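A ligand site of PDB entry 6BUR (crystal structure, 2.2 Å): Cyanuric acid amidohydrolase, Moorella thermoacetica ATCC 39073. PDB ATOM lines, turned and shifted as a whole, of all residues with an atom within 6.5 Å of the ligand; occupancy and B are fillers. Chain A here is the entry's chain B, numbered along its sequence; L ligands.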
ATOM      1  N   LYS A  41     -12.648 -30.268 -17.465  1.00  0.00           N
ATOM      2  CA  LYS A  41     -13.881 -29.795 -16.827  1.00  0.00           C
ATOM      3  C   LYS A  41     -13.505 -29.289 -15.431  1.00  0.00           C
ATOM      4  O   LYS A  41     -13.109 -30.075 -14.576  1.00  0.00           O
ATOM      5  CB  LYS A  41     -14.939 -30.899 -16.706  1.00  0.00           C
ATOM      6  CG  LYS A  41     -15.728 -31.204 -17.996  1.00  0.00           C
ATOM      7  CD  LYS A  41     -16.355 -29.975 -18.620  1.00  0.00           C
ATOM      8  CE  LYS A  41     -17.211 -29.218 -17.636  1.00  0.00           C
ATOM      9  NZ  LYS A  41     -17.894 -28.069 -18.329  1.00  0.00           N
ATOM     10  N   THR A  42     -13.626 -27.984 -15.207  1.00  0.00           N
ATOM     11  CA  THR A  42     -13.242 -27.392 -13.943  1.00  0.00           C
ATOM     12  C   THR A  42     -14.488 -26.880 -13.236  1.00  0.00           C
ATOM     13  O   THR A  42     -15.505 -26.566 -13.879  1.00  0.00           O
ATOM     14  CB  THR A  42     -12.185 -26.291 -14.172  1.00  0.00           C
ATOM     15  OG1 THR A  42     -12.743 -25.204 -14.919  1.00  0.00           O
ATOM     16  CG2 THR A  42     -10.977 -26.888 -14.974  1.00  0.00           C
ATOM     17  N   ASN A  45     -18.154 -21.734 -12.411  1.00  0.00           N
ATOM     18  CA  ASN A  45     -19.527 -21.643 -12.898  1.00  0.00           C
ATOM     19  C   ASN A  45     -19.640 -21.675 -14.422  1.00  0.00           C
ATOM     20  O   ASN A  45     -20.757 -21.635 -14.951  1.00  0.00           O
ATOM     21  CB  ASN A  45     -20.235 -20.393 -12.309  1.00  0.00           C
ATOM     22  CG  ASN A  45     -19.724 -19.040 -12.867  1.00  0.00           C
ATOM     23  OD1 ASN A  45     -19.144 -18.966 -13.957  1.00  0.00           O
ATOM     24  ND2 ASN A  45     -19.954 -17.963 -12.101  1.00  0.00           N
ATOM     25  N   GLY A  46     -18.530 -21.816 -15.138  1.00  0.00           N
ATOM     26  CA  GLY A  46     -18.590 -21.979 -16.582  1.00  0.00           C
ATOM     27  C   GLY A  46     -19.096 -20.771 -17.333  1.00  0.00           C
ATOM     28  O   GLY A  46     -19.288 -20.840 -18.562  1.00  0.00           O
ATOM     29  N   CYS A  47     -19.298 -19.649 -16.646  1.00  0.00           N
ATOM     30  CA  CYS A  47     -19.830 -18.464 -17.297  1.00  0.00           C
ATOM     31  C   CYS A  47     -18.775 -17.373 -17.400  1.00  0.00           C
ATOM     32  O   CYS A  47     -17.620 -17.634 -17.754  1.00  0.00           O
ATOM     33  CB  CYS A  47     -21.088 -17.996 -16.568  1.00  0.00           C
ATOM     34  SG  CYS A  47     -22.458 -19.231 -16.594  1.00  0.00           S
ATOM     35  N   ASP A  50     -15.689 -17.103 -14.251  1.00  0.00           N
ATOM     36  CA  ASP A  50     -15.172 -18.420 -13.877  1.00  0.00           C
ATOM     37  C   ASP A  50     -13.648 -18.331 -13.951  1.00  0.00           C
ATOM     38  O   ASP A  50     -13.083 -18.334 -15.037  1.00  0.00           O
ATOM     39  CB  ASP A  50     -15.730 -19.511 -14.801  1.00  0.00           C
ATOM     40  CG  ASP A  50     -15.327 -20.931 -14.357  1.00  0.00           C
ATOM     41  OD1 ASP A  50     -14.305 -21.124 -13.662  1.00  0.00           O
ATOM     42  OD2 ASP A  50     -16.057 -21.867 -14.718  1.00  0.00           O
ATOM     43  N   ARG A  53     -10.961 -21.871 -14.749  1.00  0.00           N
ATOM     44  CA  ARG A  53     -10.369 -22.200 -16.046  1.00  0.00           C
ATOM     45  C   ARG A  53      -8.915 -21.751 -16.100  1.00  0.00           C
ATOM     46  O   ARG A  53      -8.009 -22.548 -16.393  1.00  0.00           O
ATOM     47  CB  ARG A  53     -11.186 -21.553 -17.178  1.00  0.00           C
ATOM     48  CG  ARG A  53     -12.686 -22.004 -17.295  1.00  0.00           C
ATOM     49  CD  ARG A  53     -13.456 -21.271 -18.473  1.00  0.00           C
ATOM     50  NE  ARG A  53     -13.567 -19.840 -18.248  1.00  0.00           N
ATOM     51  CZ  ARG A  53     -14.700 -19.127 -18.234  1.00  0.00           C
ATOM     52  NH1 ARG A  53     -15.883 -19.702 -18.474  1.00  0.00           N
ATOM     53  NH2 ARG A  53     -14.639 -17.812 -17.992  1.00  0.00           N
ATOM     54  N   MET A  83      -9.894 -25.541 -20.963  1.00  0.00           N
ATOM     55  CA  MET A  83     -10.612 -25.745 -19.711  1.00  0.00           C
ATOM     56  C   MET A  83     -12.026 -25.190 -19.868  1.00  0.00           C
ATOM     57  O   MET A  83     -12.217 -23.988 -20.102  1.00  0.00           O
ATOM     58  CB  MET A  83      -9.884 -25.071 -18.548  1.00  0.00           C
ATOM     59  CG  MET A  83      -8.450 -25.578 -18.364  1.00  0.00           C
ATOM     60  SD  MET A  83      -8.309 -27.344 -17.914  1.00  0.00           S
ATOM     61  CE  MET A  83      -6.927 -27.829 -18.965  1.00  0.00           C
ATOM     62  N   SER A  84     -13.005 -26.062 -19.734  1.00  0.00           N
ATOM     63  CA  SER A  84     -14.398 -25.706 -19.792  1.00  0.00           C
ATOM     64  C   SER A  84     -14.963 -25.794 -18.376  1.00  0.00           C
ATOM     65  O   SER A  84     -15.042 -26.865 -17.778  1.00  0.00           O
ATOM     66  CB  SER A  84     -15.110 -26.628 -20.781  1.00  0.00           C
ATOM     67  OG  SER A  84     -16.495 -26.464 -20.689  1.00  0.00           O
ATOM     68  N   GLY A  85     -15.291 -24.639 -17.809  1.00  0.00           N
ATOM     69  CA  GLY A  85     -15.819 -24.593 -16.458  1.00  0.00           C
ATOM     70  C   GLY A  85     -17.262 -25.062 -16.437  1.00  0.00           C
ATOM     71  O   GLY A  85     -17.916 -25.224 -17.477  1.00  0.00           O
ATOM     72  N   GLY A  86     -17.766 -25.285 -15.235  1.00  0.00           N
ATOM     73  CA  GLY A  86     -19.148 -25.675 -15.047  1.00  0.00           C
ATOM     74  C   GLY A  86     -19.290 -27.182 -14.903  1.00  0.00           C
ATOM     75  O   GLY A  86     -19.278 -27.912 -15.895  1.00  0.00           O
ATOM     76  N   LYS A 162     -11.125 -23.868 -27.805  1.00  0.00           N
ATOM     77  CA  LYS A 162     -11.262 -22.797 -26.813  1.00  0.00           C
ATOM     78  C   LYS A 162     -11.265 -21.477 -27.571  1.00  0.00           C
ATOM     79  O   LYS A 162     -10.472 -21.277 -28.495  1.00  0.00           O
ATOM     80  CB  LYS A 162     -10.130 -22.812 -25.788  1.00  0.00           C
ATOM     81  CG  LYS A 162     -10.470 -21.971 -24.513  1.00  0.00           C
ATOM     82  CD  LYS A 162     -11.592 -22.652 -23.707  1.00  0.00           C
ATOM     83  CE  LYS A 162     -12.195 -21.778 -22.587  1.00  0.00           C
ATOM     84  NZ  LYS A 162     -13.385 -22.432 -21.844  1.00  0.00           N
ATOM     85  N   CYS A 163     -12.171 -20.589 -27.199  1.00  0.00           N
ATOM     86  CA  CYS A 163     -12.275 -19.318 -27.914  1.00  0.00           C
ATOM     87  C   CYS A 163     -12.379 -18.185 -26.910  1.00  0.00           C
ATOM     88  O   CYS A 163     -12.629 -18.408 -25.719  1.00  0.00           O
ATOM     89  CB  CYS A 163     -13.467 -19.299 -28.877  1.00  0.00           C
ATOM     90  SG  CYS A 163     -15.059 -19.756 -28.178  1.00  0.00           S
ATOM     91  N   MET A 190     -19.745 -14.586 -25.358  1.00  0.00           N
ATOM     92  CA  MET A 190     -19.356 -15.988 -25.315  1.00  0.00           C
ATOM     93  C   MET A 190     -20.117 -16.778 -26.361  1.00  0.00           C
ATOM     94  O   MET A 190     -19.545 -17.652 -27.034  1.00  0.00           O
ATOM     95  CB  MET A 190     -19.606 -16.593 -23.926  1.00  0.00           C
ATOM     96  CG  MET A 190     -18.864 -15.899 -22.746  1.00  0.00           C
ATOM     97  SD  MET A 190     -19.255 -16.686 -21.165  1.00  0.00           S
ATOM     98  CE  MET A 190     -18.385 -18.257 -21.223  1.00  0.00           C
ATOM     99  N   ARG A 194     -18.353 -18.662 -29.433  1.00  0.00           N
ATOM    100  CA  ARG A 194     -18.653 -20.073 -29.650  1.00  0.00           C
ATOM    101  C   ARG A 194     -19.266 -20.304 -31.033  1.00  0.00           C
ATOM    102  O   ARG A 194     -18.913 -21.272 -31.713  1.00  0.00           O
ATOM    103  CB  ARG A 194     -19.610 -20.609 -28.585  1.00  0.00           C
ATOM    104  CG  ARG A 194     -18.942 -20.947 -27.249  1.00  0.00           C
ATOM    105  CD  ARG A 194     -19.905 -21.610 -26.269  1.00  0.00           C
ATOM    106  NE  ARG A 194     -21.188 -20.915 -26.162  1.00  0.00           N
ATOM    107  CZ  ARG A 194     -21.601 -20.233 -25.096  1.00  0.00           C
ATOM    108  NH1 ARG A 194     -20.821 -20.113 -24.014  1.00  0.00           N
ATOM    109  NH2 ARG A 194     -22.797 -19.648 -25.113  1.00  0.00           N
ATOM    110  N   THR A 231     -17.241 -26.053 -28.886  1.00  0.00           N
ATOM    111  CA  THR A 231     -16.501 -24.815 -28.662  1.00  0.00           C
ATOM    112  C   THR A 231     -16.882 -24.255 -27.297  1.00  0.00           C
ATOM    113  O   THR A 231     -18.030 -24.355 -26.851  1.00  0.00           O
ATOM    114  CB  THR A 231     -16.784 -23.744 -29.754  1.00  0.00           C
ATOM    115  OG1 THR A 231     -18.121 -23.245 -29.611  1.00  0.00           O
ATOM    116  CG2 THR A 231     -16.616 -24.320 -31.169  1.00  0.00           C
ATOM    117  N   SER A 232     -15.894 -23.648 -26.634  1.00  0.00           N
ATOM    118  CA  SER A 232     -16.011 -23.205 -25.244  1.00  0.00           C
ATOM    119  C   SER A 232     -15.253 -21.893 -25.070  1.00  0.00           C
ATOM    120  O   SER A 232     -14.076 -21.803 -25.428  1.00  0.00           O
ATOM    121  CB  SER A 232     -15.459 -24.279 -24.290  1.00  0.00           C
ATOM    122  OG  SER A 232     -15.809 -23.987 -22.951  1.00  0.00           O
ATOM    123  N   ALA A 233     -15.914 -20.884 -24.493  1.00  0.00           N
ATOM    124  CA  ALA A 233     -15.329 -19.559 -24.336  1.00  0.00           C
ATOM    125  C   ALA A 233     -14.689 -19.389 -22.956  1.00  0.00           C
ATOM    126  O   ALA A 233     -15.068 -20.036 -21.983  1.00  0.00           O
ATOM    127  CB  ALA A 233     -16.378 -18.469 -24.562  1.00  0.00           C
ATOM    128  N   GLY A 234     -13.709 -18.480 -22.882  1.00  0.00           N
ATOM    129  CA  GLY A 234     -13.068 -18.153 -21.630  1.00  0.00           C
ATOM    130  C   GLY A 234     -12.285 -16.865 -21.722  1.00  0.00           C
ATOM    131  O   GLY A 234     -11.941 -16.395 -22.809  1.00  0.00           O
ATOM    132  N   LYS A 295     -21.973 -31.506 -26.275  1.00  0.00           N
ATOM    133  CA  LYS A 295     -22.464 -30.137 -26.165  1.00  0.00           C
ATOM    134  C   LYS A 295     -23.915 -30.142 -25.707  1.00  0.00           C
ATOM    135  O   LYS A 295     -24.701 -31.000 -26.119  1.00  0.00           O
ATOM    136  CB  LYS A 295     -22.339 -29.413 -27.521  1.00  0.00           C
ATOM    137  CG  LYS A 295     -20.896 -29.047 -27.951  1.00  0.00           C
ATOM    138  CD  LYS A 295     -20.182 -28.092 -26.944  1.00  0.00           C
ATOM    139  CE  LYS A 295     -20.978 -26.782 -26.769  1.00  0.00           C
ATOM    140  NZ  LYS A 295     -20.264 -25.731 -25.939  1.00  0.00           N
ATOM    141  N   THR A 320     -26.976 -21.874 -19.248  1.00  0.00           N
ATOM    142  CA  THR A 320     -25.942 -22.831 -19.646  1.00  0.00           C
ATOM    143  C   THR A 320     -25.585 -23.758 -18.493  1.00  0.00           C
ATOM    144  O   THR A 320     -25.195 -24.913 -18.726  1.00  0.00           O
ATOM    145  CB  THR A 320     -24.702 -22.116 -20.215  1.00  0.00           C
ATOM    146  OG1 THR A 320     -24.085 -21.282 -19.230  1.00  0.00           O
ATOM    147  CG2 THR A 320     -25.092 -21.258 -21.411  1.00  0.00           C
ATOM    148  N   ARG A 324     -26.005 -27.949 -18.889  1.00  0.00           N
ATOM    149  CA  ARG A 324     -24.930 -28.892 -18.583  1.00  0.00           C
ATOM    150  C   ARG A 324     -25.366 -29.950 -17.570  1.00  0.00           C
ATOM    151  O   ARG A 324     -25.070 -31.140 -17.753  1.00  0.00           O
ATOM    152  CB  ARG A 324     -23.693 -28.156 -18.069  1.00  0.00           C
ATOM    153  CG  ARG A 324     -22.891 -27.478 -19.184  1.00  0.00           C
ATOM    154  CD  ARG A 324     -21.590 -26.881 -18.664  1.00  0.00           C
ATOM    155  NE  ARG A 324     -21.806 -25.902 -17.620  1.00  0.00           N
ATOM    156  CZ  ARG A 324     -21.750 -24.576 -17.809  1.00  0.00           C
ATOM    157  NH1 ARG A 324     -21.451 -24.062 -19.008  1.00  0.00           N
ATOM    158  NH2 ARG A 324     -21.966 -23.778 -16.780  1.00  0.00           N
ATOM    159  N   TYR A 341     -17.241 -35.362 -20.197  1.00  0.00           N
ATOM    160  CA  TYR A 341     -17.125 -33.959 -20.590  1.00  0.00           C
ATOM    161  C   TYR A 341     -18.451 -33.447 -21.162  1.00  0.00           C
ATOM    162  O   TYR A 341     -18.905 -33.937 -22.209  1.00  0.00           O
ATOM    163  CB  TYR A 341     -16.005 -33.828 -21.618  1.00  0.00           C
ATOM    164  CG  TYR A 341     -15.809 -32.408 -22.115  1.00  0.00           C
ATOM    165  CD1 TYR A 341     -16.642 -31.879 -23.111  1.00  0.00           C
ATOM    166  CD2 TYR A 341     -14.817 -31.609 -21.600  1.00  0.00           C
ATOM    167  CE1 TYR A 341     -16.480 -30.589 -23.556  1.00  0.00           C
ATOM    168  CE2 TYR A 341     -14.646 -30.326 -22.037  1.00  0.00           C
ATOM    169  CZ  TYR A 341     -15.475 -29.824 -23.040  1.00  0.00           C
ATOM    170  OH  TYR A 341     -15.310 -28.530 -23.498  1.00  0.00           O
ATOM    171  N   VAL A 342     -19.059 -32.465 -20.504  1.00  0.00           N
ATOM    172  CA  VAL A 342     -20.234 -31.798 -21.068  1.00  0.00           C
ATOM    173  C   VAL A 342     -20.033 -30.281 -20.982  1.00  0.00           C
ATOM    174  O   VAL A 342     -19.750 -29.748 -19.897  1.00  0.00           O
ATOM    175  CB  VAL A 342     -21.543 -32.189 -20.362  1.00  0.00           C
ATOM    176  CG1 VAL A 342     -22.700 -31.382 -21.001  1.00  0.00           C
ATOM    177  CG2 VAL A 342     -21.810 -33.701 -20.509  1.00  0.00           C
ATOM    178  N   SER A 343     -20.208 -29.604 -22.109  1.00  0.00           N
ATOM    179  CA  SER A 343     -20.033 -28.162 -22.241  1.00  0.00           C
ATOM    180  C   SER A 343     -21.324 -27.527 -22.753  1.00  0.00           C
ATOM    181  O   SER A 343     -22.027 -28.101 -23.592  1.00  0.00           O
ATOM    182  CB  SER A 343     -18.840 -27.866 -23.172  1.00  0.00           C
ATOM    183  OG  SER A 343     -18.843 -26.532 -23.600  1.00  0.00           O
ATOM    184  N   GLY A 344     -21.646 -26.333 -22.219  1.00  0.00           N
ATOM    185  CA  GLY A 344     -22.889 -25.655 -22.546  1.00  0.00           C
ATOM    186  C   GLY A 344     -22.724 -24.572 -23.605  1.00  0.00           C
ATOM    187  O   GLY A 344     -21.626 -24.063 -23.860  1.00  0.00           O
ATOM    188  N   GLY A 345     -23.843 -24.182 -24.205  1.00  0.00           N
ATOM    189  CA  GLY A 345     -23.797 -23.178 -25.257  1.00  0.00           C
ATOM    190  C   GLY A 345     -23.439 -23.810 -26.588  1.00  0.00           C
ATOM    191  O   GLY A 345     -22.264 -23.870 -26.968  1.00  0.00           O
HETATM  192  N1  LIG L   1     -17.113 -21.833 -21.534  1.00  0.00           N
HETATM  193  C1  LIG L   1     -16.971 -22.570 -20.273  1.00  0.00           C
HETATM  194  O1  LIG L   1     -16.106 -22.299 -19.505  1.00  0.00           O
HETATM  195  N2  LIG L   1     -17.883 -23.698 -19.993  1.00  0.00           N
HETATM  196  C2  LIG L   1     -18.922 -24.035 -20.939  1.00  0.00           C
HETATM  197  O2  LIG L   1     -19.667 -24.930 -20.738  1.00  0.00           O
HETATM  198  C3  LIG L   1     -19.058 -23.252 -22.199  1.00  0.00           C
HETATM  199  C4  LIG L   1     -18.206 -22.137 -22.408  1.00  0.00           C
HETATM  200  O3  LIG L   1     -18.519 -21.347 -23.226  1.00  0.00           O
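The backbone carbonyl oxygen (O) of Ser 232 sits at hydrogen-bond distance from the backbone NH (N) of Cys 163 (2.9 Å).
The side-chain amino group (NZ) of Lys 162 sits at hydrogen-bond distance from the backbone carbonyl oxygen (O) of Met 83 (2.6 Å).
The backbone carbonyl oxygen (O) of Ser 84 is in hydrogen-bond range of the side-chain amino group (NZ) of Lys 41 (3.1 Å).
The side-chain amino group (NZ) of Lys 41 sits at hydrogen-bond distance from the backbone carbonyl oxygen (O) of Gly 85 (3.0 Å).
The side-chain hydroxyl of Ser 232 lies within hydrogen-bond range of the side-chain amino group of Lys 162, 3.1 Å away.
The guanidinium group (NH2) of Arg 324 lies within hydrogen-bond range of the backbone carbonyl oxygen (O) of Asn 45, 3.1 Å away.
OG of Ser 232 lies within hydrogen-bond range of OG of Ser 84, at 3.4 Å.
The guanidinium group of Arg 194 sits at hydrogen-bond distance from the backbone carbonyl oxygen of Gly 345 (3.2 Å).
A nitrogen (N2) of the ligand is in hydrogen-bond range of the backbone carbonyl oxygen (O) of Gly 85 (2.9 Å).
The side-chain hydroxyl (OG) of Ser 84 sits at hydrogen-bond distance from a nitrogen (N2) of the ligand (3.2 Å).
A nitrogen (N1) of the ligand is in hydrogen-bond range of the side-chain hydroxyl (OG) of Ser 232 (2.9 Å).
The backbone carbonyl oxygen (O) of Gly 46 sits close to a nitrogen (N2) of the ligand (3.5 Å).
An oxygen (O3) of the ligand lies within hydrogen-bond range of the guanidinium group of Arg 194 (2.7 Å).
The backbone carbonyl oxygen (O) of Ala 233 is in hydrogen-bond range of a nitrogen (N1) of the ligand.
The backbone NH of Gly 344 sits at hydrogen-bond distance from an oxygen (O2) of the ligand (2.8 Å).
The guanidinium group of Arg 324 sits at hydrogen-bond distance from an oxygen (O2) of the ligand (2.6 Å).
An oxygen (O1) of the ligand sits at hydrogen-bond distance from the guanidinium group (NH1) of Arg 53, at 2.8 Å.
The side-chain hydroxyl (OG) of Ser 343 is in hydrogen-bond range of an oxygen (O2) of the ligand (3.4 Å).
N of Ala 233 is in hydrogen-bond range of O3 of the ligand (2.9 Å).
The backbone NH (N) of Gly 85 sits at hydrogen-bond distance from an oxygen (O1) of the ligand, at 3.0 Å.
Lys 162 touches the ligand.
Met 190 touches the ligand (CE to O3, 3.7 Å).
Hydrophobic or aromatic side chains within 4 Å of the ligand: Met 190 and Ala 233.
The nearest printed residue that does not touch the ligand is Met 83 (4.3 Å).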
